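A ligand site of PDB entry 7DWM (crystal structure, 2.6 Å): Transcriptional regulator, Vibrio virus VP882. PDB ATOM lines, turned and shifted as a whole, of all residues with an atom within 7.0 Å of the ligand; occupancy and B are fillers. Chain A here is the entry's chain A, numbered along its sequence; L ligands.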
ATOM      1  N   LYS A  31      10.098 -11.283  33.161  1.00  0.00           N
ATOM      2  CA  LYS A  31       9.891 -12.279  34.202  1.00  0.00           C
ATOM      3  C   LYS A  31      11.169 -12.448  35.011  1.00  0.00           C
ATOM      4  O   LYS A  31      12.207 -11.853  34.697  1.00  0.00           O
ATOM      5  CB  LYS A  31       9.399 -13.614  33.633  1.00  0.00           C
ATOM      6  CG  LYS A  31      10.164 -14.138  32.472  1.00  0.00           C
ATOM      7  CD  LYS A  31       9.187 -14.655  31.461  1.00  0.00           C
ATOM      8  CE  LYS A  31       9.895 -15.339  30.339  1.00  0.00           C
ATOM      9  NZ  LYS A  31       8.961 -16.108  29.485  1.00  0.00           N
ATOM     10  N   PHE A  37       6.213 -14.542  35.613  1.00  0.00           N
ATOM     11  CA  PHE A  37       5.879 -13.214  35.095  1.00  0.00           C
ATOM     12  C   PHE A  37       5.875 -12.170  36.203  1.00  0.00           C
ATOM     13  O   PHE A  37       5.312 -12.394  37.275  1.00  0.00           O
ATOM     14  CB  PHE A  37       4.499 -13.248  34.434  1.00  0.00           C
ATOM     15  CG  PHE A  37       4.499 -13.743  33.012  1.00  0.00           C
ATOM     16  CD1 PHE A  37       3.314 -14.111  32.402  1.00  0.00           C
ATOM     17  CD2 PHE A  37       5.669 -13.826  32.287  1.00  0.00           C
ATOM     18  CE1 PHE A  37       3.297 -14.566  31.091  1.00  0.00           C
ATOM     19  CE2 PHE A  37       5.667 -14.268  30.984  1.00  0.00           C
ATOM     20  CZ  PHE A  37       4.476 -14.648  30.392  1.00  0.00           C
ATOM     21  N   PHE A  44       0.930  -8.451  24.912  1.00  0.00           N
ATOM     22  CA  PHE A  44       1.378  -9.817  25.164  1.00  0.00           C
ATOM     23  C   PHE A  44       0.271 -10.657  25.772  1.00  0.00           C
ATOM     24  O   PHE A  44       0.077 -11.807  25.377  1.00  0.00           O
ATOM     25  CB  PHE A  44       2.601  -9.839  26.079  1.00  0.00           C
ATOM     26  CG  PHE A  44       3.104 -11.227  26.342  1.00  0.00           C
ATOM     27  CD1 PHE A  44       2.731 -11.911  27.487  1.00  0.00           C
ATOM     28  CD2 PHE A  44       3.909 -11.874  25.418  1.00  0.00           C
ATOM     29  CE1 PHE A  44       3.174 -13.199  27.716  1.00  0.00           C
ATOM     30  CE2 PHE A  44       4.351 -13.156  25.640  1.00  0.00           C
ATOM     31  CZ  PHE A  44       3.984 -13.818  26.789  1.00  0.00           C
ATOM     32  N   LEU A  47      -1.942 -11.724  23.033  1.00  0.00           N
ATOM     33  CA  LEU A  47      -1.455 -12.706  22.074  1.00  0.00           C
ATOM     34  C   LEU A  47      -1.632 -14.120  22.619  1.00  0.00           C
ATOM     35  O   LEU A  47      -1.934 -15.061  21.874  1.00  0.00           O
ATOM     36  CB  LEU A  47       0.000 -12.428  21.732  1.00  0.00           C
ATOM     37  CG  LEU A  47       0.671 -13.402  20.774  1.00  0.00           C
ATOM     38  CD1 LEU A  47       0.300 -13.017  19.349  1.00  0.00           C
ATOM     39  CD2 LEU A  47       2.191 -13.421  20.944  1.00  0.00           C
ATOM     40  N   VAL A  48      -1.457 -14.285  23.928  1.00  0.00           N
ATOM     41  CA  VAL A  48      -1.953 -15.459  24.635  1.00  0.00           C
ATOM     42  C   VAL A  48      -3.429 -15.168  24.878  1.00  0.00           C
ATOM     43  O   VAL A  48      -3.873 -14.027  24.690  1.00  0.00           O
ATOM     44  CB  VAL A  48      -1.143 -15.698  25.921  1.00  0.00           C
ATOM     45  CG1 VAL A  48      -1.683 -16.870  26.748  1.00  0.00           C
ATOM     46  CG2 VAL A  48       0.325 -15.929  25.596  1.00  0.00           C
ATOM     47  N   ASP A  60       5.167 -19.851  32.075  1.00  0.00           N
ATOM     48  CA  ASP A  60       4.753 -19.708  30.679  1.00  0.00           C
ATOM     49  C   ASP A  60       3.609 -20.642  30.319  1.00  0.00           C
ATOM     50  O   ASP A  60       2.951 -20.433  29.294  1.00  0.00           O
ATOM     51  CB  ASP A  60       5.948 -19.911  29.753  1.00  0.00           C
ATOM     52  CG  ASP A  60       6.750 -18.648  29.559  1.00  0.00           C
ATOM     53  OD1 ASP A  60       6.149 -17.619  29.197  1.00  0.00           O
ATOM     54  OD2 ASP A  60       7.981 -18.678  29.771  1.00  0.00           O
ATOM     55  N   ASP A  62       0.604 -20.834  30.462  1.00  0.00           N
ATOM     56  CA  ASP A  62      -0.453 -19.871  30.762  1.00  0.00           C
ATOM     57  C   ASP A  62      -1.815 -20.498  30.509  1.00  0.00           C
ATOM     58  O   ASP A  62      -1.940 -21.708  30.309  1.00  0.00           O
ATOM     59  CB  ASP A  62      -0.260 -18.612  29.915  1.00  0.00           C
ATOM     60  CG  ASP A  62       0.740 -17.630  30.514  1.00  0.00           C
ATOM     61  OD1 ASP A  62       0.285 -16.658  31.139  1.00  0.00           O
ATOM     62  OD2 ASP A  62       1.972 -17.841  30.363  1.00  0.00           O
ATOM     63  N   THR A  67       0.735 -21.887  23.185  1.00  0.00           N
ATOM     64  CA  THR A  67       2.070 -21.519  23.643  1.00  0.00           C
ATOM     65  C   THR A  67       2.512 -22.364  24.830  1.00  0.00           C
ATOM     66  O   THR A  67       3.682 -22.732  24.917  1.00  0.00           O
ATOM     67  CB  THR A  67       2.111 -20.039  24.016  1.00  0.00           C
ATOM     68  OG1 THR A  67       0.883 -19.661  24.642  1.00  0.00           O
ATOM     69  CG2 THR A  67       2.303 -19.193  22.767  1.00  0.00           C
ATOM     70  N   PHE A  70       5.047 -25.282  24.828  1.00  0.00           N
ATOM     71  CA  PHE A  70       6.476 -24.997  24.773  1.00  0.00           C
ATOM     72  C   PHE A  70       6.935 -24.146  25.945  1.00  0.00           C
ATOM     73  O   PHE A  70       8.075 -23.657  25.944  1.00  0.00           O
ATOM     74  CB  PHE A  70       6.831 -24.311  23.455  1.00  0.00           C
ATOM     75  CG  PHE A  70       6.843 -25.232  22.281  1.00  0.00           C
ATOM     76  CD1 PHE A  70       8.020 -25.809  21.852  1.00  0.00           C
ATOM     77  CD2 PHE A  70       5.670 -25.542  21.613  1.00  0.00           C
ATOM     78  CE1 PHE A  70       8.046 -26.667  20.777  1.00  0.00           C
ATOM     79  CE2 PHE A  70       5.683 -26.405  20.535  1.00  0.00           C
ATOM     80  CZ  PHE A  70       6.866 -26.967  20.118  1.00  0.00           C
ATOM     81  N   PHE A  74      10.585 -22.421  26.610  1.00  0.00           N
ATOM     82  CA  PHE A  74      10.691 -20.987  26.887  1.00  0.00           C
ATOM     83  C   PHE A  74      11.616 -20.750  28.074  1.00  0.00           C
ATOM     84  O   PHE A  74      12.635 -20.051  27.960  1.00  0.00           O
ATOM     85  CB  PHE A  74       9.308 -20.392  27.178  1.00  0.00           C
ATOM     86  CG  PHE A  74       8.369 -20.389  26.012  1.00  0.00           C
ATOM     87  CD1 PHE A  74       8.777 -20.781  24.749  1.00  0.00           C
ATOM     88  CD2 PHE A  74       7.060 -19.972  26.177  1.00  0.00           C
ATOM     89  CE1 PHE A  74       7.894 -20.772  23.676  1.00  0.00           C
ATOM     90  CE2 PHE A  74       6.174 -19.947  25.119  1.00  0.00           C
ATOM     91  CZ  PHE A  74       6.593 -20.348  23.860  1.00  0.00           C
ATOM     92  N   GLN A  75      11.306 -21.379  29.217  1.00  0.00           N
ATOM     93  CA  GLN A  75      12.081 -21.089  30.411  1.00  0.00           C
ATOM     94  C   GLN A  75      13.532 -21.494  30.217  1.00  0.00           C
ATOM     95  O   GLN A  75      14.427 -20.850  30.781  1.00  0.00           O
ATOM     96  CB  GLN A  75      11.460 -21.742  31.659  1.00  0.00           C
ATOM     97  CG  GLN A  75      11.579 -23.242  31.777  1.00  0.00           C
ATOM     98  CD  GLN A  75      10.385 -23.860  32.485  1.00  0.00           C
ATOM     99  OE1 GLN A  75       9.346 -23.217  32.660  1.00  0.00           O
ATOM    100  NE2 GLN A  75      10.518 -25.117  32.885  1.00  0.00           N
ATOM    101  N   GLN A  77      15.355 -21.146  27.503  1.00  0.00           N
ATOM    102  CA  GLN A  77      15.929 -19.930  26.933  1.00  0.00           C
ATOM    103  C   GLN A  77      16.122 -18.895  28.023  1.00  0.00           C
ATOM    104  O   GLN A  77      17.203 -18.306  28.167  1.00  0.00           O
ATOM    105  CB  GLN A  77      15.018 -19.403  25.825  1.00  0.00           C
ATOM    106  CG  GLN A  77      14.571 -20.457  24.819  1.00  0.00           C
ATOM    107  CD  GLN A  77      13.270 -20.090  24.119  1.00  0.00           C
ATOM    108  OE1 GLN A  77      12.663 -19.072  24.414  1.00  0.00           O
ATOM    109  NE2 GLN A  77      12.844 -20.941  23.190  1.00  0.00           N
ATOM    110  N   ASP A  78      15.095 -18.731  28.867  1.00  0.00           N
ATOM    111  CA  ASP A  78      15.090 -17.733  29.932  1.00  0.00           C
ATOM    112  C   ASP A  78      16.260 -17.865  30.906  1.00  0.00           C
ATOM    113  O   ASP A  78      16.453 -16.966  31.729  1.00  0.00           O
ATOM    114  CB  ASP A  78      13.781 -17.812  30.711  1.00  0.00           C
ATOM    115  CG  ASP A  78      12.664 -17.091  30.018  1.00  0.00           C
ATOM    116  OD1 ASP A  78      12.818 -15.871  29.779  1.00  0.00           O
ATOM    117  OD2 ASP A  78      11.642 -17.732  29.703  1.00  0.00           O
ATOM    118  N   VAL A  90      14.515 -15.277  19.685  1.00  0.00           N
ATOM    119  CA  VAL A  90      13.777 -16.509  19.495  1.00  0.00           C
ATOM    120  C   VAL A  90      12.711 -16.336  18.430  1.00  0.00           C
ATOM    121  O   VAL A  90      11.895 -15.399  18.479  1.00  0.00           O
ATOM    122  CB  VAL A  90      13.217 -17.036  20.823  1.00  0.00           C
ATOM    123  CG1 VAL A  90      11.917 -16.416  21.122  1.00  0.00           C
ATOM    124  CG2 VAL A  90      12.982 -18.589  20.694  1.00  0.00           C
ATOM    125  N   ASP A  92       9.490 -17.668  17.292  1.00  0.00           N
ATOM    126  CA  ASP A  92       8.350 -18.347  17.878  1.00  0.00           C
ATOM    127  C   ASP A  92       7.244 -18.388  16.840  1.00  0.00           C
ATOM    128  O   ASP A  92       6.592 -17.365  16.580  1.00  0.00           O
ATOM    129  CB  ASP A  92       7.907 -17.626  19.151  1.00  0.00           C
ATOM    130  CG  ASP A  92       8.525 -18.196  20.426  1.00  0.00           C
ATOM    131  OD1 ASP A  92       8.196 -19.327  20.823  1.00  0.00           O
ATOM    132  OD2 ASP A  92       9.325 -17.518  21.067  1.00  0.00           O
ATOM    133  N   HIS A  94       3.699 -19.931  16.230  1.00  0.00           N
ATOM    134  CA  HIS A  94       2.710 -20.520  17.134  1.00  0.00           C
ATOM    135  C   HIS A  94       1.302 -20.220  16.654  1.00  0.00           C
ATOM    136  O   HIS A  94       1.062 -19.180  16.028  1.00  0.00           O
ATOM    137  CB  HIS A  94       2.880 -19.985  18.562  1.00  0.00           C
ATOM    138  CG  HIS A  94       4.083 -20.495  19.271  1.00  0.00           C
ATOM    139  ND1 HIS A  94       4.154 -21.768  19.807  1.00  0.00           N
ATOM    140  CD2 HIS A  94       5.272 -19.912  19.542  1.00  0.00           C
ATOM    141  CE1 HIS A  94       5.332 -21.941  20.366  1.00  0.00           C
ATOM    142  NE2 HIS A  94       6.038 -20.832  20.225  1.00  0.00           N
ATOM    143  N   TYR A  96      -1.249 -18.616  17.848  1.00  0.00           N
ATOM    144  CA  TYR A  96      -1.628 -17.665  18.882  1.00  0.00           C
ATOM    145  C   TYR A  96      -3.154 -17.480  18.883  1.00  0.00           C
ATOM    146  O   TYR A  96      -3.874 -17.967  18.005  1.00  0.00           O
ATOM    147  CB  TYR A  96      -0.907 -16.334  18.670  1.00  0.00           C
ATOM    148  CG  TYR A  96       0.596 -16.452  18.750  1.00  0.00           C
ATOM    149  CD1 TYR A  96       1.237 -16.744  19.949  1.00  0.00           C
ATOM    150  CD2 TYR A  96       1.394 -16.253  17.624  1.00  0.00           C
ATOM    151  CE1 TYR A  96       2.610 -16.850  20.023  1.00  0.00           C
ATOM    152  CE2 TYR A  96       2.763 -16.359  17.685  1.00  0.00           C
ATOM    153  CZ  TYR A  96       3.372 -16.654  18.887  1.00  0.00           C
ATOM    154  OH  TYR A  96       4.746 -16.760  18.961  1.00  0.00           O
ATOM    155  N   PHE A 103       6.373 -14.918  15.126  1.00  0.00           N
ATOM    156  CA  PHE A 103       6.918 -13.850  15.946  1.00  0.00           C
ATOM    157  C   PHE A 103       8.414 -14.023  16.128  1.00  0.00           C
ATOM    158  O   PHE A 103       8.962 -15.116  16.037  1.00  0.00           O
ATOM    159  CB  PHE A 103       6.238 -13.810  17.316  1.00  0.00           C
ATOM    160  CG  PHE A 103       5.122 -12.818  17.404  1.00  0.00           C
ATOM    161  CD1 PHE A 103       5.216 -11.717  18.241  1.00  0.00           C
ATOM    162  CD2 PHE A 103       3.968 -12.986  16.657  1.00  0.00           C
ATOM    163  CE1 PHE A 103       4.195 -10.798  18.327  1.00  0.00           C
ATOM    164  CE2 PHE A 103       2.934 -12.072  16.740  1.00  0.00           C
ATOM    165  CZ  PHE A 103       3.046 -10.974  17.572  1.00  0.00           C
ATOM    166  N   PHE A 105      10.743 -13.222  19.329  1.00  0.00           N
ATOM    167  CA  PHE A 105      10.815 -12.853  20.743  1.00  0.00           C
ATOM    168  C   PHE A 105      12.274 -12.660  21.124  1.00  0.00           C
ATOM    169  O   PHE A 105      13.040 -13.630  21.191  1.00  0.00           O
ATOM    170  CB  PHE A 105      10.133 -13.906  21.625  1.00  0.00           C
ATOM    171  CG  PHE A 105       8.649 -13.721  21.717  1.00  0.00           C
ATOM    172  CD1 PHE A 105       8.092 -12.907  22.683  1.00  0.00           C
ATOM    173  CD2 PHE A 105       7.801 -14.362  20.828  1.00  0.00           C
ATOM    174  CE1 PHE A 105       6.723 -12.724  22.763  1.00  0.00           C
ATOM    175  CE2 PHE A 105       6.435 -14.202  20.900  1.00  0.00           C
ATOM    176  CZ  PHE A 105       5.895 -13.375  21.876  1.00  0.00           C
ATOM    177  N   LYS A 107      14.938 -11.860  23.874  1.00  0.00           N
ATOM    178  CA  LYS A 107      15.074 -11.985  25.324  1.00  0.00           C
ATOM    179  C   LYS A 107      16.454 -11.510  25.763  1.00  0.00           C
ATOM    180  O   LYS A 107      17.479 -11.985  25.251  1.00  0.00           O
ATOM    181  CB  LYS A 107      14.813 -13.424  25.765  1.00  0.00           C
ATOM    182  CG  LYS A 107      13.537 -13.973  25.141  1.00  0.00           C
ATOM    183  CD  LYS A 107      13.389 -15.478  25.235  1.00  0.00           C
ATOM    184  CE  LYS A 107      13.056 -15.917  26.644  1.00  0.00           C
ATOM    185  NZ  LYS A 107      12.677 -17.355  26.691  1.00  0.00           N
ATOM    186  N   THR A 120      14.586 -11.635  33.102  1.00  0.00           N
ATOM    187  CA  THR A 120      14.739 -11.342  31.686  1.00  0.00           C
ATOM    188  C   THR A 120      13.623 -10.416  31.227  1.00  0.00           C
ATOM    189  O   THR A 120      12.533 -10.393  31.813  1.00  0.00           O
ATOM    190  CB  THR A 120      14.710 -12.613  30.814  1.00  0.00           C
ATOM    191  OG1 THR A 120      13.419 -13.219  30.873  1.00  0.00           O
ATOM    192  CG2 THR A 120      15.755 -13.622  31.264  1.00  0.00           C
ATOM    193  N   PHE A 122      11.502  -9.623  27.630  1.00  0.00           N
ATOM    194  CA  PHE A 122      11.187 -10.191  26.323  1.00  0.00           C
ATOM    195  C   PHE A 122      10.401  -9.178  25.510  1.00  0.00           C
ATOM    196  O   PHE A 122       9.492  -8.505  26.036  1.00  0.00           O
ATOM    197  CB  PHE A 122      10.423 -11.523  26.446  1.00  0.00           C
ATOM    198  CG  PHE A 122       9.068 -11.405  27.086  1.00  0.00           C
ATOM    199  CD1 PHE A 122       8.903 -11.724  28.424  1.00  0.00           C
ATOM    200  CD2 PHE A 122       7.959 -11.027  26.347  1.00  0.00           C
ATOM    201  CE1 PHE A 122       7.660 -11.626  29.025  1.00  0.00           C
ATOM    202  CE2 PHE A 122       6.714 -10.922  26.940  1.00  0.00           C
ATOM    203  CZ  PHE A 122       6.565 -11.222  28.280  1.00  0.00           C
ATOM    204  N   SER A 234       9.819 -22.930  18.558  1.00  0.00           N
ATOM    205  CA  SER A 234      10.508 -21.806  19.182  1.00  0.00           C
ATOM    206  C   SER A 234      11.993 -22.141  19.200  1.00  0.00           C
ATOM    207  O   SER A 234      12.399 -23.111  19.832  1.00  0.00           O
ATOM    208  CB  SER A 234      10.011 -21.559  20.601  1.00  0.00           C
ATOM    209  OG  SER A 234      10.623 -22.453  21.503  1.00  0.00           O
HETATM  210  C1  LIG L   1       7.237 -17.125  23.571  1.00  0.00           C
HETATM  211  C2  LIG L   1       6.057 -16.457  23.976  1.00  0.00           C
HETATM  212  C3  LIG L   1       7.170 -15.742  25.909  1.00  0.00           C
HETATM  213  C4  LIG L   1       8.294 -16.444  25.428  1.00  0.00           C
HETATM  214  C5  LIG L   1       4.835 -16.510  23.101  1.00  0.00           C
HETATM  215  C6  LIG L   1       7.174 -14.978  27.209  1.00  0.00           C
HETATM  216  N1  LIG L   1       8.384 -17.130  24.294  1.00  0.00           N
HETATM  217  N2  LIG L   1       6.058 -15.767  25.151  1.00  0.00           N
HETATM  218  O1  LIG L   1       9.437 -16.383  26.256  1.00  0.00           O
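The side-chain amino group of Lys 31 lies close to an oxygen (O1) of the ligand (3.3 Å). O1 of the ligand is in hydrogen-bond range of NZ of Lys 107 (3.4 Å).
NZ of Lys 31 lies within salt-bridge range of OD2 of Asp 60 (2.8 Å). The side-chain carboxylate (OD2) of Asp 78 lies within salt-bridge range of the side-chain amino group (NZ) of Lys 31, at 3.1 Å. The backbone NH (N) of Thr 120 sits at hydrogen-bond distance from the backbone carbonyl oxygen (O) of Lys 31, 2.9 Å away. The side-chain hydroxyl (OH) of Tyr 96 lies within hydrogen-bond range of the backbone carbonyl oxygen (O) of Asp 92 (3.1 Å). O of Asp 92 sits at hydrogen-bond distance from N of Phe 103 (2.9 Å). The side-chain amino group (NZ) of Lys 107 lies within salt-bridge range of the side-chain carboxylate (OD2) of Asp 78. NZ of Lys 107 sits at hydrogen-bond distance from OE1 of Gln 77 (2.9 Å). N of Phe 105 lies within hydrogen-bond range of O of Val 90.
The side-chain carboxylate of Asp 92 sits close to a nitrogen (N1) of the ligand, 3.4 Å away. Residues that only touch the ligand: Phe 44 (3.2 Å), Phe 74 (3.3 Å), Asp 60 (3.5 Å), Phe 105 (3.5 Å), Thr 67 (3.7 Å), Tyr 96 (3.8 Å) and Phe 122 (3.8 Å). Hydrophobic or aromatic side chains within 4 Å of the ligand: Phe 44, Phe 74, Tyr 96, Phe 105 and Phe 122. Of the 23 residues printed, 10 come within 4 Å of the ligand. The nearest printed residue that does not touch the ligand is Phe 37 (4.1 Å).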
